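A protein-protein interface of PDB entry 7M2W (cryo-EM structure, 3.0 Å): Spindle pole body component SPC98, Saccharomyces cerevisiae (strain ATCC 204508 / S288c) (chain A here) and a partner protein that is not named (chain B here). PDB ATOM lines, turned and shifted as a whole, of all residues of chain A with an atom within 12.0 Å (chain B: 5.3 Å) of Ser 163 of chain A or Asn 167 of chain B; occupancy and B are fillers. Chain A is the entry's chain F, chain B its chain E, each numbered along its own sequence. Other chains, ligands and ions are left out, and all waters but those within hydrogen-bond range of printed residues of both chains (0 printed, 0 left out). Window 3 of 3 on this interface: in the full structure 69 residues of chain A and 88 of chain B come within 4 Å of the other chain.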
ATOM      1  N   SER A 163      11.686 -10.126  16.902  1.00  0.00           N
ATOM      2  CA  SER A 163      12.384 -10.055  15.623  1.00  0.00           C
ATOM      3  C   SER A 163      11.867 -11.107  14.647  1.00  0.00           C
ATOM      4  O   SER A 163      12.562 -11.482  13.704  1.00  0.00           O
ATOM      5  CB  SER A 163      13.889 -10.226  15.824  1.00  0.00           C
ATOM      6  OG  SER A 163      14.571 -10.206  14.583  1.00  0.00           O
ATOM      7  N   SER A 164      10.640 -11.578  14.878  1.00  0.00           N
ATOM      8  CA  SER A 164      10.045 -12.588  14.011  1.00  0.00           C
ATOM      9  C   SER A 164       9.669 -12.051  12.637  1.00  0.00           C
ATOM     10  O   SER A 164       9.200 -12.828  11.798  1.00  0.00           O
ATOM     11  CB  SER A 164       8.809 -13.190  14.679  1.00  0.00           C
ATOM     12  OG  SER A 164       8.183 -14.135  13.830  1.00  0.00           O
ATOM     13  N   VAL A 165       9.853 -10.754  12.385  1.00  0.00           N
ATOM     14  CA  VAL A 165       9.557 -10.213  11.066  1.00  0.00           C
ATOM     15  C   VAL A 165      10.668 -10.587  10.096  1.00  0.00           C
ATOM     16  O   VAL A 165      11.849 -10.292  10.319  1.00  0.00           O
ATOM     17  CB  VAL A 165       9.350  -8.691  11.143  1.00  0.00           C
ATOM     18  CG1 VAL A 165       8.080  -8.373  11.910  1.00  0.00           C
ATOM     19  CG2 VAL A 165      10.532  -8.022  11.821  1.00  0.00           C
ATOM     20  N   THR A 166      10.296 -11.267   9.018  1.00  0.00           N
ATOM     21  CA  THR A 166      11.261 -11.652   8.002  1.00  0.00           C
ATOM     22  C   THR A 166      11.707 -10.430   7.210  1.00  0.00           C
ATOM     23  O   THR A 166      11.077  -9.372   7.242  1.00  0.00           O
ATOM     24  CB  THR A 166      10.674 -12.709   7.070  1.00  0.00           C
ATOM     25  OG1 THR A 166       9.513 -12.183   6.421  1.00  0.00           O
ATOM     26  CG2 THR A 166      10.293 -13.954   7.848  1.00  0.00           C
ATOM     27  N   LEU A 167      12.821 -10.584   6.492  1.00  0.00           N
ATOM     28  CA  LEU A 167      13.333  -9.476   5.693  1.00  0.00           C
ATOM     29  C   LEU A 167      12.393  -9.132   4.547  1.00  0.00           C
ATOM     30  O   LEU A 167      12.392  -7.991   4.071  1.00  0.00           O
ATOM     31  CB  LEU A 167      14.722  -9.805   5.159  1.00  0.00           C
ATOM     32  CG  LEU A 167      15.820  -9.972   6.206  1.00  0.00           C
ATOM     33  CD1 LEU A 167      17.118 -10.375   5.546  1.00  0.00           C
ATOM     34  CD2 LEU A 167      16.003  -8.700   7.000  1.00  0.00           C
ATOM     35  N   ARG A 168      11.591 -10.092   4.090  1.00  0.00           N
ATOM     36  CA  ARG A 168      10.590  -9.783   3.077  1.00  0.00           C
ATOM     37  C   ARG A 168       9.547  -8.813   3.616  1.00  0.00           C
ATOM     38  O   ARG A 168       9.144  -7.872   2.923  1.00  0.00           O
ATOM     39  CB  ARG A 168       9.929 -11.069   2.587  1.00  0.00           C
ATOM     40  CG  ARG A 168       8.811 -10.843   1.592  1.00  0.00           C
ATOM     41  CD  ARG A 168       9.351 -10.650   0.186  1.00  0.00           C
ATOM     42  NE  ARG A 168       8.287 -10.507  -0.802  1.00  0.00           N
ATOM     43  CZ  ARG A 168       7.471 -11.487  -1.177  1.00  0.00           C
ATOM     44  NH1 ARG A 168       7.593 -12.698  -0.652  1.00  0.00           N
ATOM     45  NH2 ARG A 168       6.533 -11.258  -2.085  1.00  0.00           N
ATOM     46  N   GLN A 169       9.104  -9.017   4.859  1.00  0.00           N
ATOM     47  CA  GLN A 169       8.116  -8.117   5.443  1.00  0.00           C
ATOM     48  C   GLN A 169       8.734  -6.772   5.787  1.00  0.00           C
ATOM     49  O   GLN A 169       8.026  -5.766   5.905  1.00  0.00           O
ATOM     50  CB  GLN A 169       7.497  -8.749   6.686  1.00  0.00           C
ATOM     51  CG  GLN A 169       6.931 -10.131   6.465  1.00  0.00           C
ATOM     52  CD  GLN A 169       6.716 -10.873   7.763  1.00  0.00           C
ATOM     53  OE1 GLN A 169       7.670 -11.304   8.409  1.00  0.00           O
ATOM     54  NE2 GLN A 169       5.459 -11.020   8.159  1.00  0.00           N
ATOM     55  N   LEU A 170      10.054  -6.733   5.965  1.00  0.00           N
ATOM     56  CA  LEU A 170      10.721  -5.456   6.177  1.00  0.00           C
ATOM     57  C   LEU A 170      10.899  -4.712   4.863  1.00  0.00           C
ATOM     58  O   LEU A 170      10.906  -3.476   4.834  1.00  0.00           O
ATOM     59  CB  LEU A 170      12.067  -5.677   6.864  1.00  0.00           C
ATOM     60  CG  LEU A 170      11.969  -6.085   8.333  1.00  0.00           C
ATOM     61  CD1 LEU A 170      13.292  -6.625   8.835  1.00  0.00           C
ATOM     62  CD2 LEU A 170      11.508  -4.911   9.182  1.00  0.00           C
ATOM     63  N   SER A 171      11.041  -5.450   3.764  1.00  0.00           N
ATOM     64  CA  SER A 171      11.253  -4.821   2.466  1.00  0.00           C
ATOM     65  C   SER A 171       9.942  -4.375   1.835  1.00  0.00           C
ATOM     66  O   SER A 171       9.916  -3.398   1.079  1.00  0.00           O
ATOM     67  CB  SER A 171      11.988  -5.783   1.538  1.00  0.00           C
ATOM     68  OG  SER A 171      12.135  -5.220   0.250  1.00  0.00           O
ATOM     69  N   ARG B  53      18.260  -3.181  10.197  1.00  0.00           N
ATOM     70  CA  ARG B  53      17.767  -4.427   9.624  1.00  0.00           C
ATOM     71  C   ARG B  53      16.832  -4.181   8.447  1.00  0.00           C
ATOM     72  O   ARG B  53      16.743  -5.018   7.548  1.00  0.00           O
ATOM     73  CB  ARG B  53      17.073  -5.273  10.685  1.00  0.00           C
ATOM     74  CG  ARG B  53      17.179  -6.755  10.406  1.00  0.00           C
ATOM     75  CD  ARG B  53      16.343  -7.574  11.358  1.00  0.00           C
ATOM     76  NE  ARG B  53      16.154  -8.924  10.846  1.00  0.00           N
ATOM     77  CZ  ARG B  53      14.994  -9.569  10.867  1.00  0.00           C
ATOM     78  NH1 ARG B  53      13.920  -8.984  11.379  1.00  0.00           N
ATOM     79  NH2 ARG B  53      14.908 -10.794  10.374  1.00  0.00           N
ATOM     80  N   VAL B 165      12.523 -17.181   6.689  1.00  0.00           N
ATOM     81  CA  VAL B 165      13.294 -17.326   7.921  1.00  0.00           C
ATOM     82  C   VAL B 165      13.420 -15.959   8.584  1.00  0.00           C
ATOM     83  O   VAL B 165      14.012 -15.044   7.997  1.00  0.00           O
ATOM     84  CB  VAL B 165      14.676 -17.936   7.650  1.00  0.00           C
ATOM     85  CG1 VAL B 165      15.525 -17.898   8.903  1.00  0.00           C
ATOM     86  CG2 VAL B 165      14.528 -19.360   7.158  1.00  0.00           C
ATOM     87  N   PRO B 166      12.891 -15.773   9.794  1.00  0.00           N
ATOM     88  CA  PRO B 166      13.209 -14.563  10.558  1.00  0.00           C
ATOM     89  C   PRO B 166      14.630 -14.632  11.088  1.00  0.00           C
ATOM     90  O   PRO B 166      15.219 -15.708  11.209  1.00  0.00           O
ATOM     91  CB  PRO B 166      12.182 -14.578  11.698  1.00  0.00           C
ATOM     92  CG  PRO B 166      11.192 -15.652  11.341  1.00  0.00           C
ATOM     93  CD  PRO B 166      11.938 -16.632  10.507  1.00  0.00           C
ATOM     94  N   ASN B 167      15.181 -13.462  11.404  1.00  0.00           N
ATOM     95  CA  ASN B 167      16.572 -13.280  11.809  1.00  0.00           C
ATOM     96  C   ASN B 167      17.553 -13.641  10.702  1.00  0.00           C
ATOM     97  O   ASN B 167      18.744 -13.826  10.978  1.00  0.00           O
ATOM     98  CB  ASN B 167      16.916 -14.071  13.077  1.00  0.00           C
ATOM     99  CG  ASN B 167      16.449 -13.377  14.343  1.00  0.00           C
ATOM    100  OD1 ASN B 167      16.657 -12.176  14.517  1.00  0.00           O
ATOM    101  ND2 ASN B 167      15.819 -14.132  15.235  1.00  0.00           N
ATOM    102  N   PHE B 168      17.088 -13.753   9.460  1.00  0.00           N
ATOM    103  CA  PHE B 168      17.989 -13.909   8.328  1.00  0.00           C
ATOM    104  C   PHE B 168      18.831 -12.650   8.171  1.00  0.00           C
ATOM    105  O   PHE B 168      18.452 -11.571   8.631  1.00  0.00           O
ATOM    106  CB  PHE B 168      17.191 -14.189   7.054  1.00  0.00           C
ATOM    107  CG  PHE B 168      18.030 -14.608   5.881  1.00  0.00           C
ATOM    108  CD1 PHE B 168      18.545 -15.888   5.799  1.00  0.00           C
ATOM    109  CD2 PHE B 168      18.291 -13.723   4.852  1.00  0.00           C
ATOM    110  CE1 PHE B 168      19.310 -16.271   4.720  1.00  0.00           C
ATOM    111  CE2 PHE B 168      19.055 -14.101   3.774  1.00  0.00           C
ATOM    112  CZ  PHE B 168      19.565 -15.375   3.707  1.00  0.00           C
ATOM    113  N   SER B 169      19.982 -12.785   7.522  1.00  0.00           N
ATOM    114  CA  SER B 169      20.925 -11.682   7.435  1.00  0.00           C
ATOM    115  C   SER B 169      21.724 -11.775   6.147  1.00  0.00           C
ATOM    116  O   SER B 169      21.503 -12.651   5.308  1.00  0.00           O
ATOM    117  CB  SER B 169      21.864 -11.669   8.642  1.00  0.00           C
ATOM    118  OG  SER B 169      22.662 -12.838   8.656  1.00  0.00           O
ATOM    119  N   GLU B 172      24.681 -14.316   6.995  1.00  0.00           N
ATOM    120  CA  GLU B 172      24.179 -15.669   6.794  1.00  0.00           C
ATOM    121  C   GLU B 172      24.053 -15.987   5.312  1.00  0.00           C
ATOM    122  O   GLU B 172      24.219 -17.140   4.906  1.00  0.00           O
ATOM    123  CB  GLU B 172      22.834 -15.846   7.495  1.00  0.00           C
ATOM    124  CG  GLU B 172      22.277 -17.252   7.400  1.00  0.00           C
ATOM    125  CD  GLU B 172      21.135 -17.495   8.363  1.00  0.00           C
ATOM    126  OE1 GLU B 172      21.004 -16.734   9.344  1.00  0.00           O
ATOM    127  OE2 GLU B 172      20.363 -18.450   8.137  1.00  0.00           O
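The guanidinium group of Arg 53 of chain B lies within hydrogen-bond range of the side-chain hydroxyl of Ser 163 of chain A (3.5 Å). O of Val 165 of chain A sits at hydrogen-bond distance from NH1 of Arg 53 of chain B (2.7 Å). The side-chain amide oxygen (OD1) of Asn 167 of chain B is in hydrogen-bond range of the side-chain hydroxyl (OG) of Ser 163 of chain A (2.9 Å).
The side-chain amide oxygen (OE1) of Gln 169 of chain A sits at hydrogen-bond distance from the backbone NH (N) of Thr 166 of chain A (2.7 Å).
Ser 163 of chain A touches Pro 166 of chain B (O to CB, 3.7 Å). O of Ser 164 of chain A touches CB of Pro 166 of chain B (3.5 Å). Thr 166 of chain A touches Val 165 of chain B. N of Pro 166 of chain B touches CG2 of Thr 166 of chain A, at 3.7 Å. Leu 167 of chain A touches Arg 53 of chain B. Phe 168 of chain B touches Leu 167 of chain A (O to CD1, 3.6 Å). Arg 53 of chain B touches Leu 170 of chain A (NH1 to CD1, 3.5 Å).
Ser 163 of chain A touches just these residues of chain B: Arg 53, Pro 166 and Asn 167. Of the printed residues of chain B, Ser 164 of chain A touches Pro 166 (3.5 Å). Printed residues of chain B within 4 Å of Thr 166 of chain A: Val 165 (3.8 Å) and Pro 166 (3.7 Å). Of the printed residues of chain B, Leu 167 of chain A touches Arg 53 (3.8 Å) and Phe 168 (3.6 Å). Of the printed residues of chain B, Leu 170 of chain A touches Arg 53 (3.5 Å). Pro 166 of chain B touches just these residues of chain A: Ser 163, Ser 164 and Thr 166. Of chain A, only Leu 167 comes within 4 Å of Phe 168 of chain B. Ser 169 of chain B touches none of the printed residues of chain A. The nearest residue of chain A that does not touch Asn 167 of chain B is Val 165 of chain A (4.7 Å).
Of the 7 printed residues of chain B, 5 touch a printed residue of chain A. Hydrophobic or aromatic side chains of chain B within 4 Å of the printed part of chain A: Pro 166 and Phe 168. Of the 9 printed residues of chain A, 6 touch a printed residue of chain B. Hydrophobic or aromatic side chains of chain A that line the printed part of chain B: Val 165, Leu 167 and Leu 170. Among the printed residues, 10 pairs touch across the chains. Among the printed residues, no Asp or Glu carboxylate lies within 4 Å of a Lys or Arg side-chain nitrogen of the other chain.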
